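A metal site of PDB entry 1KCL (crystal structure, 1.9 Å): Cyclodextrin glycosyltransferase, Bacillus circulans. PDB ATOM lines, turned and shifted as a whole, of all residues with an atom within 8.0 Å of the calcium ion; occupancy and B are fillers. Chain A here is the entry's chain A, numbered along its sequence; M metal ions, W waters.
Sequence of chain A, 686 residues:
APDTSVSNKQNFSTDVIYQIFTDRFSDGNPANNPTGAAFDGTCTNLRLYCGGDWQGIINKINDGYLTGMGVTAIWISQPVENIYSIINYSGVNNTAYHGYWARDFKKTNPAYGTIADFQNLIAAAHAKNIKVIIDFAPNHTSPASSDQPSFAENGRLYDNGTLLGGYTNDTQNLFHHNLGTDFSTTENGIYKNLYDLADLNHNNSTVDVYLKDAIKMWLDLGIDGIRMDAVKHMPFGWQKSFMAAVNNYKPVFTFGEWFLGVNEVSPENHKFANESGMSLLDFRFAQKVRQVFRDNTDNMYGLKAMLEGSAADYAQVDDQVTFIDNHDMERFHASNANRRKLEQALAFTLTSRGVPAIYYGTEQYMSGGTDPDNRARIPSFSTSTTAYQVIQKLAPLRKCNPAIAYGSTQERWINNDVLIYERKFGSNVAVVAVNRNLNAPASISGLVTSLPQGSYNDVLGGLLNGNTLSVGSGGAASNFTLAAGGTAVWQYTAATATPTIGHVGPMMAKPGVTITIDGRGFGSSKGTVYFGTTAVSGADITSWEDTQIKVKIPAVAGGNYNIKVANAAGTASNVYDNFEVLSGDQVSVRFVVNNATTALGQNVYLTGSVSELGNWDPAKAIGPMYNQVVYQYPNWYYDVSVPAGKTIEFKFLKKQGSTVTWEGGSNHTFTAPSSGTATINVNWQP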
ATOM      1  N   PRO A 138      22.431 -22.351 -26.928  1.00  0.00           N
ATOM      2  CA  PRO A 138      21.829 -21.459 -25.933  1.00  0.00           C
ATOM      3  C   PRO A 138      20.302 -21.410 -25.942  1.00  0.00           C
ATOM      4  O   PRO A 138      19.700 -20.551 -25.299  1.00  0.00           O
ATOM      5  CB  PRO A 138      22.447 -20.116 -26.290  1.00  0.00           C
ATOM      6  CG  PRO A 138      22.500 -20.178 -27.794  1.00  0.00           C
ATOM      7  CD  PRO A 138      23.027 -21.582 -28.041  1.00  0.00           C
ATOM      8  N   ASN A 139      19.649 -22.325 -26.668  1.00  0.00           N
ATOM      9  CA  ASN A 139      18.193 -22.344 -26.722  1.00  0.00           C
ATOM     10  C   ASN A 139      17.593 -22.960 -25.469  1.00  0.00           C
ATOM     11  O   ASN A 139      16.514 -22.574 -25.028  1.00  0.00           O
ATOM     12  CB  ASN A 139      17.704 -23.150 -27.929  1.00  0.00           C
ATOM     13  CG  ASN A 139      16.188 -23.335 -27.935  1.00  0.00           C
ATOM     14  OD1 ASN A 139      15.442 -22.373 -28.128  1.00  0.00           O
ATOM     15  ND2 ASN A 139      15.734 -24.565 -27.707  1.00  0.00           N
ATOM     16  N   HIS A 140      18.310 -23.911 -24.884  1.00  0.00           N
ATOM     17  CA  HIS A 140      17.803 -24.630 -23.725  1.00  0.00           C
ATOM     18  C   HIS A 140      18.933 -25.152 -22.847  1.00  0.00           C
ATOM     19  O   HIS A 140      20.117 -24.959 -23.152  1.00  0.00           O
ATOM     20  CB  HIS A 140      17.017 -25.837 -24.214  1.00  0.00           C
ATOM     21  CG  HIS A 140      17.793 -26.702 -25.165  1.00  0.00           C
ATOM     22  ND1 HIS A 140      17.905 -26.407 -26.514  1.00  0.00           N
ATOM     23  CD2 HIS A 140      18.579 -27.781 -24.950  1.00  0.00           C
ATOM     24  CE1 HIS A 140      18.734 -27.269 -27.076  1.00  0.00           C
ATOM     25  NE2 HIS A 140      19.153 -28.108 -26.148  1.00  0.00           N
ATOM     26  N   HIS A 176      11.070 -20.610 -20.128  1.00  0.00           N
ATOM     27  CA  HIS A 176       9.722 -20.404 -20.670  1.00  0.00           C
ATOM     28  C   HIS A 176       8.827 -21.490 -20.099  1.00  0.00           C
ATOM     29  O   HIS A 176       9.248 -22.640 -19.951  1.00  0.00           O
ATOM     30  CB  HIS A 176       9.728 -20.506 -22.193  1.00  0.00           C
ATOM     31  CG  HIS A 176      10.171 -19.250 -22.878  1.00  0.00           C
ATOM     32  ND1 HIS A 176      10.836 -19.266 -24.090  1.00  0.00           N
ATOM     33  CD2 HIS A 176      10.020 -17.951 -22.548  1.00  0.00           C
ATOM     34  CE1 HIS A 176      11.073 -18.021 -24.473  1.00  0.00           C
ATOM     35  NE2 HIS A 176      10.582 -17.201 -23.554  1.00  0.00           N
ATOM     36  N   GLU A 187       6.748 -18.593 -34.337  1.00  0.00           N
ATOM     37  CA  GLU A 187       6.584 -18.089 -32.969  1.00  0.00           C
ATOM     38  C   GLU A 187       6.374 -19.241 -31.996  1.00  0.00           C
ATOM     39  O   GLU A 187       6.952 -19.255 -30.913  1.00  0.00           O
ATOM     40  CB  GLU A 187       5.390 -17.135 -32.887  1.00  0.00           C
ATOM     41  CG  GLU A 187       4.876 -16.916 -31.465  1.00  0.00           C
ATOM     42  CD  GLU A 187       3.654 -16.028 -31.398  1.00  0.00           C
ATOM     43  OE1 GLU A 187       2.852 -16.039 -32.351  1.00  0.00           O
ATOM     44  OE2 GLU A 187       3.496 -15.323 -30.381  1.00  0.00           O
ATOM     45  N   ASN A 188       5.535 -20.186 -32.387  1.00  0.00           N
ATOM     46  CA  ASN A 188       5.232 -21.349 -31.562  1.00  0.00           C
ATOM     47  C   ASN A 188       6.509 -22.137 -31.291  1.00  0.00           C
ATOM     48  O   ASN A 188       6.746 -22.606 -30.166  1.00  0.00           O
ATOM     49  CB  ASN A 188       4.192 -22.233 -32.260  1.00  0.00           C
ATOM     50  CG  ASN A 188       3.781 -23.439 -31.431  1.00  0.00           C
ATOM     51  OD1 ASN A 188       4.529 -24.418 -31.320  1.00  0.00           O
ATOM     52  ND2 ASN A 188       2.600 -23.367 -30.834  1.00  0.00           N
ATOM     53  N   GLY A 189       7.357 -22.261 -32.313  1.00  0.00           N
ATOM     54  CA  GLY A 189       8.596 -22.992 -32.161  1.00  0.00           C
ATOM     55  C   GLY A 189       9.656 -22.259 -31.365  1.00  0.00           C
ATOM     56  O   GLY A 189      10.610 -22.863 -30.886  1.00  0.00           O
ATOM     57  N   ILE A 190       9.477 -20.946 -31.201  1.00  0.00           N
ATOM     58  CA  ILE A 190      10.452 -20.143 -30.457  1.00  0.00           C
ATOM     59  C   ILE A 190      10.156 -20.006 -28.965  1.00  0.00           C
ATOM     60  O   ILE A 190      11.044 -20.164 -28.143  1.00  0.00           O
ATOM     61  CB  ILE A 190      10.563 -18.716 -31.055  1.00  0.00           C
ATOM     62  CG1 ILE A 190      11.172 -18.771 -32.449  1.00  0.00           C
ATOM     63  CG2 ILE A 190      11.404 -17.838 -30.132  1.00  0.00           C
ATOM     64  CD1 ILE A 190      11.214 -17.431 -33.159  1.00  0.00           C
ATOM     65  N   TYR A 191       8.901 -19.714 -28.630  1.00  0.00           N
ATOM     66  CA  TYR A 191       8.547 -19.471 -27.232  1.00  0.00           C
ATOM     67  C   TYR A 191       7.996 -20.645 -26.426  1.00  0.00           C
ATOM     68  O   TYR A 191       7.561 -20.480 -25.292  1.00  0.00           O
ATOM     69  CB  TYR A 191       7.608 -18.272 -27.172  1.00  0.00           C
ATOM     70  CG  TYR A 191       8.293 -17.013 -27.649  1.00  0.00           C
ATOM     71  CD1 TYR A 191       9.219 -16.346 -26.831  1.00  0.00           C
ATOM     72  CD2 TYR A 191       8.095 -16.526 -28.945  1.00  0.00           C
ATOM     73  CE1 TYR A 191       9.920 -15.235 -27.297  1.00  0.00           C
ATOM     74  CE2 TYR A 191       8.789 -15.408 -29.417  1.00  0.00           C
ATOM     75  CZ  TYR A 191       9.704 -14.769 -28.584  1.00  0.00           C
ATOM     76  OH  TYR A 191      10.404 -13.679 -29.038  1.00  0.00           O
ATOM     77  N   LYS A 192       8.024 -21.834 -27.027  1.00  0.00           N
ATOM     78  CA  LYS A 192       7.596 -23.046 -26.340  1.00  0.00           C
ATOM     79  C   LYS A 192       8.784 -23.997 -26.316  1.00  0.00           C
ATOM     80  O   LYS A 192       9.733 -23.823 -27.089  1.00  0.00           O
ATOM     81  CB  LYS A 192       6.408 -23.687 -27.077  1.00  0.00           C
ATOM     82  CG  LYS A 192       5.137 -22.839 -27.046  1.00  0.00           C
ATOM     83  CD  LYS A 192       3.989 -23.553 -27.745  1.00  0.00           C
ATOM     84  CE  LYS A 192       2.685 -22.768 -27.623  1.00  0.00           C
ATOM     85  NZ  LYS A 192       2.225 -22.645 -26.207  1.00  0.00           N
ATOM     86  N   ASN A 193       8.745 -24.991 -25.423  1.00  0.00           N
ATOM     87  CA  ASN A 193       9.848 -25.931 -25.313  1.00  0.00           C
ATOM     88  C   ASN A 193      10.041 -26.804 -26.540  1.00  0.00           C
ATOM     89  O   ASN A 193       9.072 -27.248 -27.167  1.00  0.00           O
ATOM     90  CB  ASN A 193       9.664 -26.852 -24.097  1.00  0.00           C
ATOM     91  CG  ASN A 193       9.612 -26.094 -22.778  1.00  0.00           C
ATOM     92  OD1 ASN A 193      10.253 -25.058 -22.620  1.00  0.00           O
ATOM     93  ND2 ASN A 193       8.867 -26.632 -21.832  1.00  0.00           N
ATOM     94  N   LEU A 194      11.300 -27.033 -26.897  1.00  0.00           N
ATOM     95  CA  LEU A 194      11.638 -27.905 -28.009  1.00  0.00           C
ATOM     96  C   LEU A 194      11.630 -29.296 -27.379  1.00  0.00           C
ATOM     97  O   LEU A 194      12.578 -29.688 -26.703  1.00  0.00           O
ATOM     98  CB  LEU A 194      13.034 -27.570 -28.535  1.00  0.00           C
ATOM     99  CG  LEU A 194      13.507 -28.289 -29.791  1.00  0.00           C
ATOM    100  CD1 LEU A 194      12.551 -28.020 -30.941  1.00  0.00           C
ATOM    101  CD2 LEU A 194      14.919 -27.834 -30.143  1.00  0.00           C
ATOM    102  N   LEU A 197      12.905 -30.168 -23.586  1.00  0.00           N
ATOM    103  CA  LEU A 197      14.062 -29.365 -23.210  1.00  0.00           C
ATOM    104  C   LEU A 197      13.637 -28.039 -22.573  1.00  0.00           C
ATOM    105  O   LEU A 197      12.836 -27.307 -23.150  1.00  0.00           O
ATOM    106  CB  LEU A 197      14.941 -29.096 -24.426  1.00  0.00           C
ATOM    107  CG  LEU A 197      15.513 -30.329 -25.141  1.00  0.00           C
ATOM    108  CD1 LEU A 197      16.138 -29.912 -26.460  1.00  0.00           C
ATOM    109  CD2 LEU A 197      16.529 -31.021 -24.240  1.00  0.00           C
ATOM    110  N   ALA A 198      14.182 -27.733 -21.399  1.00  0.00           N
ATOM    111  CA  ALA A 198      13.873 -26.489 -20.680  1.00  0.00           C
ATOM    112  C   ALA A 198      14.278 -25.277 -21.515  1.00  0.00           C
ATOM    113  O   ALA A 198      15.458 -24.957 -21.637  1.00  0.00           O
ATOM    114  CB  ALA A 198      14.595 -26.471 -19.343  1.00  0.00           C
ATOM    115  N   ASP A 199      13.279 -24.593 -22.077  1.00  0.00           N
ATOM    116  CA  ASP A 199      13.510 -23.436 -22.931  1.00  0.00           C
ATOM    117  C   ASP A 199      13.980 -22.199 -22.164  1.00  0.00           C
ATOM    118  O   ASP A 199      13.258 -21.674 -21.312  1.00  0.00           O
ATOM    119  CB  ASP A 199      12.227 -23.106 -23.714  1.00  0.00           C
ATOM    120  CG  ASP A 199      12.508 -22.451 -25.040  1.00  0.00           C
ATOM    121  OD1 ASP A 199      13.174 -23.086 -25.894  1.00  0.00           O
ATOM    122  OD2 ASP A 199      12.062 -21.298 -25.255  1.00  0.00           O
ATOM    123  N   LEU A 200      15.184 -21.742 -22.467  1.00  0.00           N
ATOM    124  CA  LEU A 200      15.732 -20.553 -21.805  1.00  0.00           C
ATOM    125  C   LEU A 200      14.986 -19.294 -22.241  1.00  0.00           C
ATOM    126  O   LEU A 200      14.593 -19.156 -23.404  1.00  0.00           O
ATOM    127  CB  LEU A 200      17.226 -20.409 -22.117  1.00  0.00           C
ATOM    128  CG  LEU A 200      18.152 -21.375 -21.369  1.00  0.00           C
ATOM    129  CD1 LEU A 200      19.561 -21.289 -21.933  1.00  0.00           C
ATOM    130  CD2 LEU A 200      18.140 -21.034 -19.885  1.00  0.00           C
ATOM    131  N   ASN A 201      14.794 -18.381 -21.292  1.00  0.00           N
ATOM    132  CA  ASN A 201      14.122 -17.111 -21.542  1.00  0.00           C
ATOM    133  C   ASN A 201      15.169 -16.022 -21.711  1.00  0.00           C
ATOM    134  O   ASN A 201      15.688 -15.484 -20.738  1.00  0.00           O
ATOM    135  CB  ASN A 201      13.176 -16.782 -20.371  1.00  0.00           C
ATOM    136  CG  ASN A 201      12.587 -15.380 -20.466  1.00  0.00           C
ATOM    137  OD1 ASN A 201      12.539 -14.789 -21.542  1.00  0.00           O
ATOM    138  ND2 ASN A 201      12.137 -14.862 -19.334  1.00  0.00           N
ATOM    139  N   HIS A 202      15.475 -15.689 -22.968  1.00  0.00           N
ATOM    140  CA  HIS A 202      16.486 -14.692 -23.274  1.00  0.00           C
ATOM    141  C   HIS A 202      16.054 -13.258 -22.976  1.00  0.00           C
ATOM    142  O   HIS A 202      16.862 -12.333 -23.077  1.00  0.00           O
ATOM    143  CB  HIS A 202      16.922 -14.818 -24.727  1.00  0.00           C
ATOM    144  CG  HIS A 202      17.461 -16.168 -25.072  1.00  0.00           C
ATOM    145  ND1 HIS A 202      16.665 -17.191 -25.550  1.00  0.00           N
ATOM    146  CD2 HIS A 202      18.713 -16.686 -24.956  1.00  0.00           C
ATOM    147  CE1 HIS A 202      17.401 -18.286 -25.707  1.00  0.00           C
ATOM    148  NE2 HIS A 202      18.644 -18.003 -25.363  1.00  0.00           N
ATOM    149  N   ALA A 230      19.772 -24.998 -33.078  1.00  0.00           N
ATOM    150  CA  ALA A 230      18.368 -24.609 -33.137  1.00  0.00           C
ATOM    151  C   ALA A 230      18.117 -23.104 -33.191  1.00  0.00           C
ATOM    152  O   ALA A 230      17.406 -22.571 -32.343  1.00  0.00           O
ATOM    153  CB  ALA A 230      17.614 -25.210 -31.950  1.00  0.00           C
ATOM    154  N   VAL A 231      18.685 -22.439 -34.194  1.00  0.00           N
ATOM    155  CA  VAL A 231      18.524 -20.986 -34.316  1.00  0.00           C
ATOM    156  C   VAL A 231      17.112 -20.582 -34.732  1.00  0.00           C
ATOM    157  O   VAL A 231      16.707 -19.426 -34.543  1.00  0.00           O
ATOM    158  CB  VAL A 231      19.542 -20.396 -35.314  1.00  0.00           C
ATOM    159  CG1 VAL A 231      20.961 -20.691 -34.846  1.00  0.00           C
ATOM    160  CG2 VAL A 231      19.304 -20.943 -36.714  1.00  0.00           C
ATOM    161  N   LYS A 232      16.356 -21.519 -35.280  1.00  0.00           N
ATOM    162  CA  LYS A 232      14.979 -21.225 -35.680  1.00  0.00           C
ATOM    163  C   LYS A 232      14.065 -21.218 -34.447  1.00  0.00           C
ATOM    164  O   LYS A 232      12.896 -20.843 -34.541  1.00  0.00           O
ATOM    165  CB  LYS A 232      14.469 -22.260 -36.690  1.00  0.00           C
ATOM    166  CG  LYS A 232      13.085 -21.942 -37.208  1.00  0.00           C
ATOM    167  CD  LYS A 232      12.534 -23.027 -38.120  1.00  0.00           C
ATOM    168  CE  LYS A 232      11.149 -22.652 -38.622  1.00  0.00           C
ATOM    169  NZ  LYS A 232      10.553 -23.716 -39.481  1.00  0.00           N
ATOM    170  N   HIS A 233      14.611 -21.630 -33.310  1.00  0.00           N
ATOM    171  CA  HIS A 233      13.834 -21.734 -32.073  1.00  0.00           C
ATOM    172  C   HIS A 233      14.182 -20.708 -30.997  1.00  0.00           C
ATOM    173  O   HIS A 233      13.796 -20.852 -29.840  1.00  0.00           O
ATOM    174  CB  HIS A 233      13.952 -23.154 -31.516  1.00  0.00           C
ATOM    175  CG  HIS A 233      13.476 -24.199 -32.479  1.00  0.00           C
ATOM    176  ND1 HIS A 233      12.153 -24.340 -32.827  1.00  0.00           N
ATOM    177  CD2 HIS A 233      14.149 -25.113 -33.210  1.00  0.00           C
ATOM    178  CE1 HIS A 233      12.032 -25.301 -33.735  1.00  0.00           C
ATOM    179  NE2 HIS A 233      13.228 -25.786 -33.981  1.00  0.00           N
ATOM    180  N   MET A 234      14.915 -19.670 -31.378  1.00  0.00           N
ATOM    181  CA  MET A 234      15.273 -18.592 -30.460  1.00  0.00           C
ATOM    182  C   MET A 234      14.887 -17.273 -31.127  1.00  0.00           C
ATOM    183  O   MET A 234      14.826 -17.185 -32.360  1.00  0.00           O
ATOM    184  CB  MET A 234      16.780 -18.590 -30.174  1.00  0.00           C
ATOM    185  CG  MET A 234      17.267 -19.822 -29.446  1.00  0.00           C
ATOM    186  SD  MET A 234      19.022 -19.734 -29.026  1.00  0.00           S
ATOM    187  CE  MET A 234      19.741 -20.415 -30.516  1.00  0.00           C
ATOM    188  N   PRO A 235      14.602 -16.230 -30.321  1.00  0.00           N
ATOM    189  CA  PRO A 235      14.227 -14.936 -30.895  1.00  0.00           C
ATOM    190  C   PRO A 235      15.310 -14.438 -31.848  1.00  0.00           C
ATOM    191  O   PRO A 235      16.474 -14.294 -31.460  1.00  0.00           O
ATOM    192  CB  PRO A 235      14.079 -14.038 -29.666  1.00  0.00           C
ATOM    193  CG  PRO A 235      13.674 -15.008 -28.584  1.00  0.00           C
ATOM    194  CD  PRO A 235      14.586 -16.181 -28.852  1.00  0.00           C
HETATM  195 CA    CA M   1      13.401 -21.298 -27.569  1.00  0.00          CA
HETATM  196  O   HOH W   1      13.293 -18.833 -27.437  1.00  0.00           O
HETATM  197  O   HOH W   2      14.989 -20.505 -25.890  1.00  0.00           O
HETATM  198  O   HOH W   3      12.009 -23.093 -28.461  1.00  0.00           O
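ND2 of Asn 139 sits at hydrogen-bond distance from ND1 of His 140 (3.1 Å). The side-chain sulfur of Met 234 sits at hydrogen-bond distance from the backbone NH of Asn 139 (3.6 Å). A ring nitrogen (ND1) of His 233 is in hydrogen-bond range of the backbone carbonyl oxygen of Gly 189 (2.9 Å). The backbone carbonyl oxygen (O) of Asp 199 sits at hydrogen-bond distance from the backbone NH (N) of His 176 (2.7 Å). N of Leu 200 is in hydrogen-bond range of O of Asn 139 (3.0 Å). The backbone NH (N) of Asp 199 lies close to the side-chain amide oxygen (OD1) of Asn 193, 3.1 Å away.
Within 4 Å of the calcium ion: Asn 139, Ile 190, Asp 199 and His 233.
The backbone carbonyl oxygen (O) of His 233 binds the calcium ion (2.3 Å). The calcium ion is bound by the side-chain amide oxygen (OD1) of Asn 139. Water W3 binds the calcium ion, 2.4 Å away. Water W2 is bound to the calcium ion (2.4 Å). The side-chain carboxylate (OD1) of Asp 199 is bound to the calcium ion, at 2.5 Å. Water W1 binds the calcium ion (2.5 Å). OD2 of Asp 199 binds the calcium ion. The calcium ion is bound by O of Ile 190 (2.7 Å).
Water W2 bridges O of Asn 139 (2.7 Å) and O of Leu 200 (2.9 Å).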
